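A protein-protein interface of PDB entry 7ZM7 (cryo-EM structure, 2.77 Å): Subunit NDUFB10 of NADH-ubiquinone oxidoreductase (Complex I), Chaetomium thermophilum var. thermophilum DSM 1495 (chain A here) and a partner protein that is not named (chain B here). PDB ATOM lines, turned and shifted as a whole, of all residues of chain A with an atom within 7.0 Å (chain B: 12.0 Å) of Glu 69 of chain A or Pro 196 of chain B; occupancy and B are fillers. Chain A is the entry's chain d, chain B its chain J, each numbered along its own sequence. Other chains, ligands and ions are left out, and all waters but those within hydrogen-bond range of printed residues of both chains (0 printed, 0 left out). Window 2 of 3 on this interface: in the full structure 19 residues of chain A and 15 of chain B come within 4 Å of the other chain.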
ATOM      1  N   GLU A  63      19.859 -20.846 -32.055  1.00  0.00           N
ATOM      2  CA  GLU A  63      19.304 -22.132 -32.442  1.00  0.00           C
ATOM      3  C   GLU A  63      18.605 -22.107 -33.788  1.00  0.00           C
ATOM      4  O   GLU A  63      18.534 -23.140 -34.455  1.00  0.00           O
ATOM      5  CB  GLU A  63      18.344 -22.633 -31.366  1.00  0.00           C
ATOM      6  CG  GLU A  63      18.835 -22.412 -29.953  1.00  0.00           C
ATOM      7  CD  GLU A  63      20.071 -23.203 -29.609  1.00  0.00           C
ATOM      8  OE1 GLU A  63      20.446 -24.108 -30.378  1.00  0.00           O
ATOM      9  OE2 GLU A  63      20.668 -22.921 -28.549  1.00  0.00           O
ATOM     10  N   VAL A  65      16.390 -22.645 -36.589  1.00  0.00           N
ATOM     11  CA  VAL A  65      15.198 -23.454 -36.804  1.00  0.00           C
ATOM     12  C   VAL A  65      14.800 -24.165 -35.516  1.00  0.00           C
ATOM     13  O   VAL A  65      13.610 -24.300 -35.205  1.00  0.00           O
ATOM     14  CB  VAL A  65      15.408 -24.443 -37.963  1.00  0.00           C
ATOM     15  CG1 VAL A  65      16.503 -25.426 -37.654  1.00  0.00           C
ATOM     16  CG2 VAL A  65      14.124 -25.159 -38.263  1.00  0.00           C
ATOM     17  N   ASN A  66      15.784 -24.597 -34.731  1.00  0.00           N
ATOM     18  CA  ASN A  66      15.554 -25.333 -33.501  1.00  0.00           C
ATOM     19  C   ASN A  66      15.187 -24.436 -32.333  1.00  0.00           C
ATOM     20  O   ASN A  66      15.211 -24.903 -31.197  1.00  0.00           O
ATOM     21  CB  ASN A  66      16.790 -26.163 -33.151  1.00  0.00           C
ATOM     22  CG  ASN A  66      17.142 -27.173 -34.226  1.00  0.00           C
ATOM     23  OD1 ASN A  66      16.342 -28.031 -34.569  1.00  0.00           O
ATOM     24  ND2 ASN A  66      18.336 -27.059 -34.772  1.00  0.00           N
ATOM     25  N   HIS A  67      14.857 -23.165 -32.557  1.00  0.00           N
ATOM     26  CA  HIS A  67      14.415 -22.329 -31.445  1.00  0.00           C
ATOM     27  C   HIS A  67      13.137 -22.854 -30.809  1.00  0.00           C
ATOM     28  O   HIS A  67      12.930 -22.652 -29.613  1.00  0.00           O
ATOM     29  CB  HIS A  67      14.209 -20.883 -31.895  1.00  0.00           C
ATOM     30  CG  HIS A  67      12.868 -20.623 -32.496  1.00  0.00           C
ATOM     31  ND1 HIS A  67      11.823 -20.084 -31.781  1.00  0.00           N
ATOM     32  CD2 HIS A  67      12.396 -20.843 -33.742  1.00  0.00           C
ATOM     33  CE1 HIS A  67      10.763 -19.983 -32.561  1.00  0.00           C
ATOM     34  NE2 HIS A  67      11.086 -20.431 -33.758  1.00  0.00           N
ATOM     35  N   LEU A  68      12.312 -23.564 -31.561  1.00  0.00           N
ATOM     36  CA  LEU A  68      11.016 -24.024 -31.096  1.00  0.00           C
ATOM     37  C   LEU A  68      11.108 -25.128 -30.057  1.00  0.00           C
ATOM     38  O   LEU A  68      10.080 -25.535 -29.515  1.00  0.00           O
ATOM     39  CB  LEU A  68      10.174 -24.493 -32.284  1.00  0.00           C
ATOM     40  CG  LEU A  68       9.276 -23.426 -32.890  1.00  0.00           C
ATOM     41  CD1 LEU A  68       8.769 -23.800 -34.255  1.00  0.00           C
ATOM     42  CD2 LEU A  68       8.134 -23.238 -31.963  1.00  0.00           C
ATOM     43  N   GLU A  69      12.307 -25.620 -29.770  1.00  0.00           N
ATOM     44  CA  GLU A  69      12.493 -26.666 -28.783  1.00  0.00           C
ATOM     45  C   GLU A  69      13.509 -26.330 -27.716  1.00  0.00           C
ATOM     46  O   GLU A  69      13.457 -26.933 -26.642  1.00  0.00           O
ATOM     47  CB  GLU A  69      12.926 -27.961 -29.469  1.00  0.00           C
ATOM     48  CG  GLU A  69      14.174 -27.812 -30.303  1.00  0.00           C
ATOM     49  CD  GLU A  69      15.443 -28.002 -29.494  1.00  0.00           C
ATOM     50  OE1 GLU A  69      15.378 -28.649 -28.427  1.00  0.00           O
ATOM     51  OE2 GLU A  69      16.501 -27.496 -29.923  1.00  0.00           O
ATOM     52  N   LYS A  70      14.425 -25.399 -27.957  1.00  0.00           N
ATOM     53  CA  LYS A  70      15.574 -25.221 -27.089  1.00  0.00           C
ATOM     54  C   LYS A  70      15.443 -24.026 -26.156  1.00  0.00           C
ATOM     55  O   LYS A  70      16.229 -23.908 -25.213  1.00  0.00           O
ATOM     56  CB  LYS A  70      16.842 -25.082 -27.946  1.00  0.00           C
ATOM     57  CG  LYS A  70      18.155 -25.068 -27.186  1.00  0.00           C
ATOM     58  CD  LYS A  70      18.371 -26.387 -26.466  1.00  0.00           C
ATOM     59  CE  LYS A  70      18.525 -27.531 -27.452  1.00  0.00           C
ATOM     60  NZ  LYS A  70      19.784 -27.426 -28.235  1.00  0.00           N
ATOM     61  N   CYS A  71      14.454 -23.164 -26.371  1.00  0.00           N
ATOM     62  CA  CYS A  71      14.349 -21.906 -25.643  1.00  0.00           C
ATOM     63  C   CYS A  71      13.025 -21.770 -24.889  1.00  0.00           C
ATOM     64  O   CYS A  71      12.594 -20.659 -24.584  1.00  0.00           O
ATOM     65  CB  CYS A  71      14.547 -20.730 -26.600  1.00  0.00           C
ATOM     66  SG  CYS A  71      15.916 -20.909 -27.763  1.00  0.00           S
ATOM     67  N   GLY A  72      12.377 -22.891 -24.561  1.00  0.00           N
ATOM     68  CA  GLY A  72      11.068 -22.824 -23.935  1.00  0.00           C
ATOM     69  C   GLY A  72      11.075 -22.460 -22.463  1.00  0.00           C
ATOM     70  O   GLY A  72      10.110 -21.872 -21.968  1.00  0.00           O
ATOM     71  N   LYS A  73      12.130 -22.827 -21.737  1.00  0.00           N
ATOM     72  CA  LYS A  73      12.234 -22.406 -20.348  1.00  0.00           C
ATOM     73  C   LYS A  73      12.343 -20.896 -20.251  1.00  0.00           C
ATOM     74  O   LYS A  73      11.705 -20.271 -19.399  1.00  0.00           O
ATOM     75  CB  LYS A  73      13.434 -23.079 -19.687  1.00  0.00           C
ATOM     76  CG  LYS A  73      13.470 -22.941 -18.179  1.00  0.00           C
ATOM     77  CD  LYS A  73      14.511 -23.858 -17.567  1.00  0.00           C
ATOM     78  CE  LYS A  73      15.913 -23.319 -17.782  1.00  0.00           C
ATOM     79  NZ  LYS A  73      16.932 -24.136 -17.072  1.00  0.00           N
ATOM     80  N   ARG A  75      11.178 -18.982 -22.554  1.00  0.00           N
ATOM     81  CA  ARG A  75       9.855 -18.542 -22.966  1.00  0.00           C
ATOM     82  C   ARG A  75       8.885 -18.564 -21.800  1.00  0.00           C
ATOM     83  O   ARG A  75       8.097 -17.632 -21.622  1.00  0.00           O
ATOM     84  CB  ARG A  75       9.332 -19.422 -24.091  1.00  0.00           C
ATOM     85  CG  ARG A  75       9.865 -19.080 -25.434  1.00  0.00           C
ATOM     86  CD  ARG A  75       9.014 -19.694 -26.477  1.00  0.00           C
ATOM     87  NE  ARG A  75       8.932 -21.135 -26.308  1.00  0.00           N
ATOM     88  CZ  ARG A  75       9.595 -22.015 -27.047  1.00  0.00           C
ATOM     89  NH1 ARG A  75       9.440 -23.307 -26.820  1.00  0.00           N
ATOM     90  NH2 ARG A  75      10.403 -21.606 -28.011  1.00  0.00           N
ATOM     91  N   PRO B 191      -5.065 -22.067 -20.673  1.00  0.00           N
ATOM     92  CA  PRO B 191      -3.992 -21.501 -21.500  1.00  0.00           C
ATOM     93  C   PRO B 191      -2.869 -22.510 -21.777  1.00  0.00           C
ATOM     94  O   PRO B 191      -2.659 -23.388 -20.957  1.00  0.00           O
ATOM     95  CB  PRO B 191      -3.475 -20.309 -20.683  1.00  0.00           C
ATOM     96  CG  PRO B 191      -3.898 -20.614 -19.264  1.00  0.00           C
ATOM     97  CD  PRO B 191      -5.207 -21.364 -19.398  1.00  0.00           C
ATOM     98  N   VAL B 192      -2.170 -22.360 -22.904  1.00  0.00           N
ATOM     99  CA  VAL B 192      -1.143 -23.361 -23.325  1.00  0.00           C
ATOM    100  C   VAL B 192       0.140 -23.183 -22.506  1.00  0.00           C
ATOM    101  O   VAL B 192       0.459 -22.030 -22.159  1.00  0.00           O
ATOM    102  CB  VAL B 192      -0.900 -23.287 -24.844  1.00  0.00           C
ATOM    103  CG1 VAL B 192      -2.100 -23.792 -25.628  1.00  0.00           C
ATOM    104  CG2 VAL B 192      -0.516 -21.887 -25.295  1.00  0.00           C
ATOM    105  N   CYS B 193       0.834 -24.286 -22.189  1.00  0.00           N
ATOM    106  CA  CYS B 193       2.033 -24.224 -21.357  1.00  0.00           C
ATOM    107  C   CYS B 193       3.128 -23.381 -21.990  1.00  0.00           C
ATOM    108  O   CYS B 193       3.859 -22.684 -21.278  1.00  0.00           O
ATOM    109  CB  CYS B 193       2.553 -25.633 -21.082  1.00  0.00           C
ATOM    110  SG  CYS B 193       3.995 -25.678 -20.004  1.00  0.00           S
ATOM    111  N   ALA B 194       3.267 -23.442 -23.316  1.00  0.00           N
ATOM    112  CA  ALA B 194       4.266 -22.669 -24.058  1.00  0.00           C
ATOM    113  C   ALA B 194       5.690 -23.018 -23.646  1.00  0.00           C
ATOM    114  O   ALA B 194       6.565 -22.153 -23.639  1.00  0.00           O
ATOM    115  CB  ALA B 194       4.029 -21.162 -23.920  1.00  0.00           C
ATOM    116  N   ASP B 195       5.915 -24.286 -23.291  1.00  0.00           N
ATOM    117  CA  ASP B 195       7.214 -24.836 -22.909  1.00  0.00           C
ATOM    118  C   ASP B 195       7.139 -26.350 -23.096  1.00  0.00           C
ATOM    119  O   ASP B 195       6.306 -27.007 -22.447  1.00  0.00           O
ATOM    120  CB  ASP B 195       7.569 -24.486 -21.466  1.00  0.00           C
ATOM    121  CG  ASP B 195       8.902 -25.062 -21.029  1.00  0.00           C
ATOM    122  OD1 ASP B 195       9.770 -25.296 -21.891  1.00  0.00           O
ATOM    123  OD2 ASP B 195       9.086 -25.272 -19.812  1.00  0.00           O
ATOM    124  N   PRO B 196       7.974 -26.939 -23.957  1.00  0.00           N
ATOM    125  CA  PRO B 196       7.784 -28.363 -24.284  1.00  0.00           C
ATOM    126  C   PRO B 196       8.101 -29.317 -23.145  1.00  0.00           C
ATOM    127  O   PRO B 196       7.720 -30.492 -23.215  1.00  0.00           O
ATOM    128  CB  PRO B 196       8.729 -28.569 -25.470  1.00  0.00           C
ATOM    129  CG  PRO B 196       9.787 -27.554 -25.278  1.00  0.00           C
ATOM    130  CD  PRO B 196       9.128 -26.358 -24.664  1.00  0.00           C
ATOM    131  N   ASP B 197       8.785 -28.863 -22.103  1.00  0.00           N
ATOM    132  CA  ASP B 197       9.153 -29.719 -20.983  1.00  0.00           C
ATOM    133  C   ASP B 197       8.509 -29.188 -19.711  1.00  0.00           C
ATOM    134  O   ASP B 197       8.731 -28.031 -19.338  1.00  0.00           O
ATOM    135  CB  ASP B 197      10.671 -29.794 -20.835  1.00  0.00           C
ATOM    136  CG  ASP B 197      11.330 -30.485 -22.005  1.00  0.00           C
ATOM    137  OD1 ASP B 197      10.652 -31.302 -22.662  1.00  0.00           O
ATOM    138  OD2 ASP B 197      12.515 -30.208 -22.276  1.00  0.00           O
ATOM    139  N   GLN B 198       7.724 -30.035 -19.051  1.00  0.00           N
ATOM    140  CA  GLN B 198       7.027 -29.672 -17.820  1.00  0.00           C
ATOM    141  C   GLN B 198       6.167 -28.426 -17.999  1.00  0.00           C
ATOM    142  O   GLN B 198       6.341 -27.435 -17.292  1.00  0.00           O
ATOM    143  CB  GLN B 198       8.026 -29.460 -16.681  1.00  0.00           C
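The side-chain carboxylate of Asp 195 of chain B lies close to the backbone carbonyl oxygen of Gly 72 of chain A.
The side-chain carboxylate (OD1) of Asp 195 of chain B sits at hydrogen-bond distance from the backbone NH (N) of Lys 73 of chain A (3.4 Å).
NZ of Lys 70 of chain A lies within salt-bridge range of OE2 of Glu 69 of chain A (3.7 Å).
O of His 67 of chain A lies within hydrogen-bond range of NH2 of Arg 75 of chain A (3.2 Å).
SG of Cys 193 of chain B lies within hydrogen-bond range of O of Asp 195 of chain B.
Among the printed residues, pairs that only touch across the chains: Glu 69 of chain A with Pro 196 of chain B (3.96 Å), Gly 72 of chain A with Ala 194 of chain B (3.9 Å), Arg 75 of chain A with Ala 194 of chain B (3.7 Å) and Arg 75 of chain A with Pro 196 of chain B (3.7 Å).
No residue of chain B comes within 4 Å of Glu 63 of chain A.
No residue of chain B comes within 4 Å of His 67 of chain A.
No residue of chain B comes within 4 Å of Leu 68 of chain A.
Of chain B, only Pro 196 comes within 4 Å of Glu 69 of chain A.
No residue of chain B comes within 4 Å of Lys 70 of chain A.
Of the printed residues of chain B, Gly 72 of chain A touches Ala 194 and Asp 195.
Of the printed residues of chain B, Lys 73 of chain A touches Asp 195.
Printed residues of chain A within 4 Å of Asp 195 of chain B: Gly 72 and Lys 73.
Pro 196 of chain B touches two residues of chain A.
The nearest printed residue of chain A that does not touch Ala 194 of chain B is Lys 73 of chain A (5.9 Å).
Hydrophobic or aromatic side chains of chain B within 4 Å of the printed part of chain A: Pro 196.
Of the 11 printed residues of chain A, 4 touch a printed residue of chain B.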
